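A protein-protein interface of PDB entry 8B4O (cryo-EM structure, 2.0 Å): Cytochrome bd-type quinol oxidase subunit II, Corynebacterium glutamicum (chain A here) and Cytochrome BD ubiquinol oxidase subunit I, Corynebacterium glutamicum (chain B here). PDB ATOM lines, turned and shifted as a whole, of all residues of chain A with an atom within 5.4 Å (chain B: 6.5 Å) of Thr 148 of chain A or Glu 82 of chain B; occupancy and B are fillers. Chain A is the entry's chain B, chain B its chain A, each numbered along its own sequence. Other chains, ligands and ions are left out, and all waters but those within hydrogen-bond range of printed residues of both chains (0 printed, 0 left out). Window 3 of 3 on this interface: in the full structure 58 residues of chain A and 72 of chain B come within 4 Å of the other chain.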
ATOM      1  N   ALA A  76       4.734 -21.681 -27.055  1.00  0.00           N
ATOM      2  CA  ALA A  76       5.190 -22.946 -27.613  1.00  0.00           C
ATOM      3  C   ALA A  76       5.301 -24.024 -26.545  1.00  0.00           C
ATOM      4  O   ALA A  76       4.787 -25.133 -26.727  1.00  0.00           O
ATOM      5  CB  ALA A  76       6.525 -22.745 -28.322  1.00  0.00           C
ATOM      6  N   THR A  77       5.947 -23.717 -25.417  1.00  0.00           N
ATOM      7  CA  THR A  77       6.151 -24.725 -24.383  1.00  0.00           C
ATOM      8  C   THR A  77       4.829 -25.191 -23.788  1.00  0.00           C
ATOM      9  O   THR A  77       4.594 -26.396 -23.646  1.00  0.00           O
ATOM     10  CB  THR A  77       7.068 -24.174 -23.290  1.00  0.00           C
ATOM     11  OG1 THR A  77       8.234 -23.606 -23.894  1.00  0.00           O
ATOM     12  CG2 THR A  77       7.494 -25.276 -22.346  1.00  0.00           C
ATOM     13  N   PRO A 142       7.685 -30.872 -16.618  1.00  0.00           N
ATOM     14  CA  PRO A 142       9.046 -31.333 -16.924  1.00  0.00           C
ATOM     15  C   PRO A 142       9.708 -30.524 -18.028  1.00  0.00           C
ATOM     16  O   PRO A 142       9.750 -30.948 -19.187  1.00  0.00           O
ATOM     17  CB  PRO A 142       8.840 -32.793 -17.348  1.00  0.00           C
ATOM     18  CG  PRO A 142       7.487 -33.160 -16.849  1.00  0.00           C
ATOM     19  CD  PRO A 142       6.681 -31.913 -16.885  1.00  0.00           C
ATOM     20  N   ILE A 143      10.230 -29.354 -17.666  1.00  0.00           N
ATOM     21  CA  ILE A 143      10.802 -28.437 -18.645  1.00  0.00           C
ATOM     22  C   ILE A 143      12.306 -28.644 -18.718  1.00  0.00           C
ATOM     23  O   ILE A 143      13.001 -28.652 -17.696  1.00  0.00           O
ATOM     24  CB  ILE A 143      10.461 -26.994 -18.266  1.00  0.00           C
ATOM     25  CG1 ILE A 143       8.955 -26.852 -18.151  1.00  0.00           C
ATOM     26  CG2 ILE A 143      10.982 -26.037 -19.318  1.00  0.00           C
ATOM     27  CD1 ILE A 143       8.575 -25.701 -17.348  1.00  0.00           C
ATOM     28  N   LYS A 144      12.817 -28.800 -19.931  1.00  0.00           N
ATOM     29  CA  LYS A 144      14.214 -29.127 -20.140  1.00  0.00           C
ATOM     30  C   LYS A 144      15.051 -27.853 -20.245  1.00  0.00           C
ATOM     31  O   LYS A 144      14.575 -26.740 -20.014  1.00  0.00           O
ATOM     32  CB  LYS A 144      14.352 -29.999 -21.384  1.00  0.00           C
ATOM     33  CG  LYS A 144      13.738 -31.373 -21.203  1.00  0.00           C
ATOM     34  CD  LYS A 144      13.899 -32.245 -22.431  1.00  0.00           C
ATOM     35  CE  LYS A 144      13.245 -33.597 -22.205  1.00  0.00           C
ATOM     36  NZ  LYS A 144      13.361 -34.491 -23.385  1.00  0.00           N
ATOM     37  N   ASP A 146      16.288 -26.741 -23.031  1.00  0.00           N
ATOM     38  CA  ASP A 146      15.846 -26.068 -24.242  1.00  0.00           C
ATOM     39  C   ASP A 146      14.397 -25.601 -24.170  1.00  0.00           C
ATOM     40  O   ASP A 146      13.797 -25.341 -25.218  1.00  0.00           O
ATOM     41  CB  ASP A 146      16.045 -26.986 -25.452  1.00  0.00           C
ATOM     42  CG  ASP A 146      15.414 -28.351 -25.263  1.00  0.00           C
ATOM     43  OD1 ASP A 146      15.799 -29.284 -25.998  1.00  0.00           O
ATOM     44  OD2 ASP A 146      14.547 -28.503 -24.378  1.00  0.00           O
ATOM     45  N   HIS A 147      13.830 -25.499 -22.968  1.00  0.00           N
ATOM     46  CA  HIS A 147      12.477 -24.983 -22.757  1.00  0.00           C
ATOM     47  C   HIS A 147      11.421 -25.847 -23.441  1.00  0.00           C
ATOM     48  O   HIS A 147      10.395 -25.343 -23.895  1.00  0.00           O
ATOM     49  CB  HIS A 147      12.351 -23.531 -23.233  1.00  0.00           C
ATOM     50  CG  HIS A 147      13.517 -22.665 -22.867  1.00  0.00           C
ATOM     51  ND1 HIS A 147      13.619 -22.027 -21.651  1.00  0.00           N
ATOM     52  CD2 HIS A 147      14.618 -22.310 -23.572  1.00  0.00           C
ATOM     53  CE1 HIS A 147      14.739 -21.327 -21.616  1.00  0.00           C
ATOM     54  NE2 HIS A 147      15.363 -21.483 -22.769  1.00  0.00           N
ATOM     55  N   THR A 148      11.656 -27.153 -23.517  1.00  0.00           N
ATOM     56  CA  THR A 148      10.765 -28.065 -24.216  1.00  0.00           C
ATOM     57  C   THR A 148      10.277 -29.151 -23.266  1.00  0.00           C
ATOM     58  O   THR A 148      11.036 -29.688 -22.457  1.00  0.00           O
ATOM     59  CB  THR A 148      11.465 -28.691 -25.433  1.00  0.00           C
ATOM     60  OG1 THR A 148      11.556 -27.723 -26.483  1.00  0.00           O
ATOM     61  CG2 THR A 148      10.701 -29.895 -25.947  1.00  0.00           C
ATOM     62  N   ILE A 149       8.985 -29.461 -23.369  1.00  0.00           N
ATOM     63  CA  ILE A 149       8.340 -30.498 -22.574  1.00  0.00           C
ATOM     64  C   ILE A 149       8.099 -31.710 -23.461  1.00  0.00           C
ATOM     65  O   ILE A 149       7.677 -31.572 -24.615  1.00  0.00           O
ATOM     66  CB  ILE A 149       7.021 -30.001 -21.954  1.00  0.00           C
ATOM     67  CG1 ILE A 149       7.263 -28.751 -21.114  1.00  0.00           C
ATOM     68  CG2 ILE A 149       6.389 -31.081 -21.111  1.00  0.00           C
ATOM     69  CD1 ILE A 149       6.000 -28.147 -20.567  1.00  0.00           C
ATOM     70  N   ASP A 150       8.384 -32.901 -22.923  1.00  0.00           N
ATOM     71  CA  ASP A 150       8.233 -34.131 -23.696  1.00  0.00           C
ATOM     72  C   ASP A 150       6.777 -34.410 -24.052  1.00  0.00           C
ATOM     73  O   ASP A 150       6.489 -34.856 -25.169  1.00  0.00           O
ATOM     74  CB  ASP A 150       8.825 -35.305 -22.920  1.00  0.00           C
ATOM     75  CG  ASP A 150       9.058 -36.521 -23.789  1.00  0.00           C
ATOM     76  OD1 ASP A 150       8.939 -36.406 -25.024  1.00  0.00           O
ATOM     77  OD2 ASP A 150       9.358 -37.597 -23.235  1.00  0.00           O
ATOM     78  N   GLY B  77       1.059 -23.516 -31.899  1.00  0.00           N
ATOM     79  CA  GLY B  77       1.967 -23.864 -30.823  1.00  0.00           C
ATOM     80  C   GLY B  77       1.879 -25.308 -30.379  1.00  0.00           C
ATOM     81  O   GLY B  77       2.853 -25.850 -29.850  1.00  0.00           O
ATOM     82  N   ASN B  79       1.659 -27.982 -32.343  1.00  0.00           N
ATOM     83  CA  ASN B  79       2.348 -28.912 -33.227  1.00  0.00           C
ATOM     84  C   ASN B  79       3.646 -28.376 -33.809  1.00  0.00           C
ATOM     85  O   ASN B  79       4.421 -29.161 -34.364  1.00  0.00           O
ATOM     86  CB  ASN B  79       1.424 -29.323 -34.377  1.00  0.00           C
ATOM     87  CG  ASN B  79       0.324 -30.255 -33.931  1.00  0.00           C
ATOM     88  OD1 ASN B  79      -0.826 -29.849 -33.782  1.00  0.00           O
ATOM     89  ND2 ASN B  79       0.668 -31.516 -33.725  1.00  0.00           N
ATOM     90  N   TRP B  80       3.906 -27.075 -33.702  1.00  0.00           N
ATOM     91  CA  TRP B  80       5.035 -26.432 -34.371  1.00  0.00           C
ATOM     92  C   TRP B  80       5.758 -25.511 -33.392  1.00  0.00           C
ATOM     93  O   TRP B  80       5.989 -24.336 -33.667  1.00  0.00           O
ATOM     94  CB  TRP B  80       4.559 -25.688 -35.616  1.00  0.00           C
ATOM     95  CG  TRP B  80       3.760 -26.577 -36.500  1.00  0.00           C
ATOM     96  CD1 TRP B  80       2.411 -26.745 -36.491  1.00  0.00           C
ATOM     97  CD2 TRP B  80       4.271 -27.479 -37.475  1.00  0.00           C
ATOM     98  NE1 TRP B  80       2.045 -27.676 -37.425  1.00  0.00           N
ATOM     99  CE2 TRP B  80       3.174 -28.144 -38.042  1.00  0.00           C
ATOM    100  CE3 TRP B  80       5.553 -27.776 -37.938  1.00  0.00           C
ATOM    101  CZ2 TRP B  80       3.317 -29.086 -39.049  1.00  0.00           C
ATOM    102  CZ3 TRP B  80       5.693 -28.713 -38.935  1.00  0.00           C
ATOM    103  CH2 TRP B  80       4.585 -29.359 -39.480  1.00  0.00           C
ATOM    104  N   SER B  81       6.102 -26.058 -32.223  1.00  0.00           N
ATOM    105  CA  SER B  81       6.621 -25.239 -31.131  1.00  0.00           C
ATOM    106  C   SER B  81       7.915 -24.537 -31.511  1.00  0.00           C
ATOM    107  O   SER B  81       8.111 -23.371 -31.165  1.00  0.00           O
ATOM    108  CB  SER B  81       6.846 -26.090 -29.887  1.00  0.00           C
ATOM    109  OG  SER B  81       7.969 -26.936 -30.046  1.00  0.00           O
ATOM    110  N   GLU B  82       8.829 -25.235 -32.183  1.00  0.00           N
ATOM    111  CA  GLU B  82      10.099 -24.612 -32.546  1.00  0.00           C
ATOM    112  C   GLU B  82       9.879 -23.464 -33.523  1.00  0.00           C
ATOM    113  O   GLU B  82      10.477 -22.390 -33.388  1.00  0.00           O
ATOM    114  CB  GLU B  82      11.039 -25.662 -33.129  1.00  0.00           C
ATOM    115  CG  GLU B  82      11.452 -26.713 -32.122  1.00  0.00           C
ATOM    116  CD  GLU B  82      12.307 -26.150 -31.009  1.00  0.00           C
ATOM    117  OE1 GLU B  82      13.063 -25.190 -31.265  1.00  0.00           O
ATOM    118  OE2 GLU B  82      12.220 -26.664 -29.874  1.00  0.00           O
ATOM    119  N   TYR B  83       9.015 -23.679 -34.517  1.00  0.00           N
ATOM    120  CA  TYR B  83       8.498 -22.579 -35.323  1.00  0.00           C
ATOM    121  C   TYR B  83       7.861 -21.495 -34.470  1.00  0.00           C
ATOM    122  O   TYR B  83       8.149 -20.307 -34.642  1.00  0.00           O
ATOM    123  CB  TYR B  83       7.484 -23.110 -36.329  1.00  0.00           C
ATOM    124  CG  TYR B  83       6.770 -22.018 -37.072  1.00  0.00           C
ATOM    125  CD1 TYR B  83       7.400 -21.284 -38.058  1.00  0.00           C
ATOM    126  CD2 TYR B  83       5.454 -21.706 -36.758  1.00  0.00           C
ATOM    127  CE1 TYR B  83       6.732 -20.284 -38.722  1.00  0.00           C
ATOM    128  CE2 TYR B  83       4.784 -20.711 -37.411  1.00  0.00           C
ATOM    129  CZ  TYR B  83       5.426 -20.005 -38.393  1.00  0.00           C
ATOM    130  OH  TYR B  83       4.756 -19.008 -39.046  1.00  0.00           O
ATOM    131  N   SER B  84       6.986 -21.884 -33.548  1.00  0.00           N
ATOM    132  CA  SER B  84       6.265 -20.907 -32.743  1.00  0.00           C
ATOM    133  C   SER B  84       7.215 -20.108 -31.860  1.00  0.00           C
ATOM    134  O   SER B  84       6.842 -19.064 -31.315  1.00  0.00           O
ATOM    135  CB  SER B  84       5.216 -21.633 -31.908  1.00  0.00           C
ATOM    136  OG  SER B  84       4.512 -20.741 -31.083  1.00  0.00           O
ATOM    137  N   ARG B  85       8.445 -20.596 -31.695  1.00  0.00           N
ATOM    138  CA  ARG B  85       9.457 -19.871 -30.940  1.00  0.00           C
ATOM    139  C   ARG B  85      10.279 -18.980 -31.852  1.00  0.00           C
ATOM    140  O   ARG B  85      10.642 -17.860 -31.479  1.00  0.00           O
ATOM    141  CB  ARG B  85      10.373 -20.851 -30.218  1.00  0.00           C
ATOM    142  CG  ARG B  85       9.742 -21.523 -29.041  1.00  0.00           C
ATOM    143  CD  ARG B  85      10.740 -22.371 -28.299  1.00  0.00           C
ATOM    144  NE  ARG B  85      10.149 -22.909 -27.084  1.00  0.00           N
ATOM    145  CZ  ARG B  85       9.611 -24.114 -27.000  1.00  0.00           C
ATOM    146  NH1 ARG B  85       9.600 -24.905 -28.060  1.00  0.00           N
ATOM    147  NH2 ARG B  85       9.088 -24.530 -25.860  1.00  0.00           N
ATOM    148  N   PHE B  86      10.592 -19.470 -33.049  1.00  0.00           N
ATOM    149  CA  PHE B  86      11.476 -18.732 -33.936  1.00  0.00           C
ATOM    150  C   PHE B  86      10.823 -17.470 -34.476  1.00  0.00           C
ATOM    151  O   PHE B  86      11.520 -16.498 -34.783  1.00  0.00           O
ATOM    152  CB  PHE B  86      11.917 -19.632 -35.082  1.00  0.00           C
ATOM    153  CG  PHE B  86      12.931 -19.007 -35.980  1.00  0.00           C
ATOM    154  CD1 PHE B  86      14.245 -18.880 -35.575  1.00  0.00           C
ATOM    155  CD2 PHE B  86      12.574 -18.549 -37.232  1.00  0.00           C
ATOM    156  CE1 PHE B  86      15.179 -18.308 -36.399  1.00  0.00           C
ATOM    157  CE2 PHE B  86      13.505 -17.977 -38.060  1.00  0.00           C
ATOM    158  CZ  PHE B  86      14.808 -17.856 -37.643  1.00  0.00           C
ATOM    159  N   VAL B  87       9.499 -17.459 -34.600  1.00  0.00           N
ATOM    160  CA  VAL B  87       8.806 -16.371 -35.272  1.00  0.00           C
ATOM    161  C   VAL B  87       7.794 -15.661 -34.388  1.00  0.00           C
ATOM    162  O   VAL B  87       7.275 -14.613 -34.799  1.00  0.00           O
ATOM    163  CB  VAL B  87       8.119 -16.864 -36.561  1.00  0.00           C
ATOM    164  CG1 VAL B  87       9.111 -17.580 -37.433  1.00  0.00           C
ATOM    165  CG2 VAL B  87       6.963 -17.773 -36.217  1.00  0.00           C
ATOM    166  N   MET B 429      13.914 -21.076 -41.878  1.00  0.00           N
ATOM    167  CA  MET B 429      13.640 -22.256 -41.069  1.00  0.00           C
ATOM    168  C   MET B 429      12.991 -23.306 -41.959  1.00  0.00           C
ATOM    169  O   MET B 429      12.256 -22.965 -42.887  1.00  0.00           O
ATOM    170  CB  MET B 429      12.729 -21.926 -39.875  1.00  0.00           C
ATOM    171  CG  MET B 429      12.311 -23.139 -39.050  1.00  0.00           C
ATOM    172  SD  MET B 429      11.762 -22.787 -37.371  1.00  0.00           S
ATOM    173  CE  MET B 429      13.332 -22.640 -36.523  1.00  0.00           C
ATOM    174  N   MET B 433      12.757 -28.744 -38.691  1.00  0.00           N
ATOM    175  CA  MET B 433      13.323 -28.048 -37.545  1.00  0.00           C
ATOM    176  C   MET B 433      12.308 -27.194 -36.802  1.00  0.00           C
ATOM    177  O   MET B 433      12.655 -26.604 -35.777  1.00  0.00           O
ATOM    178  CB  MET B 433      14.496 -27.172 -37.994  1.00  0.00           C
ATOM    179  CG  MET B 433      15.683 -27.957 -38.523  1.00  0.00           C
ATOM    180  SD  MET B 433      16.406 -29.073 -37.308  1.00  0.00           S
ATOM    181  CE  MET B 433      17.134 -27.904 -36.164  1.00  0.00           C
ATOM    182  N   GLY B 434      11.075 -27.107 -37.288  1.00  0.00           N
ATOM    183  CA  GLY B 434      10.082 -26.257 -36.665  1.00  0.00           C
ATOM    184  C   GLY B 434       8.995 -27.017 -35.943  1.00  0.00           C
ATOM    185  O   GLY B 434       8.184 -26.421 -35.233  1.00  0.00           O
ATOM    186  N   VAL B 435       8.972 -28.339 -36.108  1.00  0.00           N
ATOM    187  CA  VAL B 435       7.904 -29.148 -35.537  1.00  0.00           C
ATOM    188  C   VAL B 435       8.189 -29.409 -34.065  1.00  0.00           C
ATOM    189  O   VAL B 435       9.345 -29.586 -33.657  1.00  0.00           O
ATOM    190  CB  VAL B 435       7.745 -30.460 -36.322  1.00  0.00           C
ATOM    191  CG1 VAL B 435       8.976 -31.338 -36.169  1.00  0.00           C
ATOM    192  CG2 VAL B 435       6.492 -31.199 -35.884  1.00  0.00           C
ATOM    193  N   SER B 436       7.138 -29.395 -33.252  1.00  0.00           N
ATOM    194  CA  SER B 436       7.272 -29.813 -31.866  1.00  0.00           C
ATOM    195  C   SER B 436       7.393 -31.329 -31.794  1.00  0.00           C
ATOM    196  O   SER B 436       6.610 -32.059 -32.406  1.00  0.00           O
ATOM    197  CB  SER B 436       6.079 -29.335 -31.044  1.00  0.00           C
ATOM    198  OG  SER B 436       4.897 -30.006 -31.413  1.00  0.00           O
ATOM    199  N   ASP B 437       8.384 -31.803 -31.046  1.00  0.00           N
ATOM    200  CA  ASP B 437       8.678 -33.230 -30.987  1.00  0.00           C
ATOM    201  C   ASP B 437       7.641 -33.913 -30.103  1.00  0.00           C
ATOM    202  O   ASP B 437       7.593 -33.681 -28.891  1.00  0.00           O
ATOM    203  CB  ASP B 437      10.093 -33.457 -30.464  1.00  0.00           C
ATOM    204  CG  ASP B 437      10.539 -34.898 -30.592  1.00  0.00           C
ATOM    205  OD1 ASP B 437       9.803 -35.704 -31.195  1.00  0.00           O
ATOM    206  OD2 ASP B 437      11.634 -35.226 -30.092  1.00  0.00           O
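NH2 of Arg 85 of chain B lies within hydrogen-bond range of O of His 147 of chain A (2.5 Å).
NH2 of Arg 85 of chain B sits close to OG1 of Thr 77 of chain A, 2.3 Å away.
O of His 147 of chain A lies within hydrogen-bond range of OG1 of Thr 77 of chain A (2.8 Å).
N of Thr 148 of chain A sits close to OD2 of Asp 146 of chain A (3.3 Å).
OG of Ser 81 of chain B sits at hydrogen-bond distance from NH1 of Arg 85 of chain B.
OE2 of Glu 82 of chain B is in salt-bridge range of NH1 of Arg 85 of chain B.
N of Glu 82 of chain B lies within hydrogen-bond range of O of Gly 434 of chain B, 3.3 Å away.
Among the printed residues, pairs that only touch across the chains: Ala 76 of chain A with Ser 81 of chain B, Ala 76 of chain A with Arg 85 of chain B, Thr 148 of chain A with Glu 82 of chain B, Ala 76 of chain A with Gly 77 of chain B, Thr 148 of chain A with Arg 85 of chain B and Ala 76 of chain A with Ser 84 of chain B.
Thr 148 of chain A touches just these residues of chain B: Glu 82 and Arg 85.
Of chain A, only Thr 148 comes within 4 Å of Glu 82 of chain B.
Of the printed residues of chain A, Ser 84 of chain B touches Ala 76.
Of the printed residues of chain B, Ala 76 of chain A touches Gly 77, Ser 81, Ser 84 and Arg 85.
Ile 143 of chain A touches none of the printed residues of chain B.
Lys 144 of chain A touches none of the printed residues of chain B.
The nearest residue of chain B that does not touch Thr 148 of chain A is Ser 81 of chain B (5.1 Å).
Printed residues of chain A that touch a printed residue of chain B: Ala 76, Thr 77, His 147 and Thr 148.
Hydrophobic or aromatic side chains of chain A that line the printed part of chain B: Ala 76.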
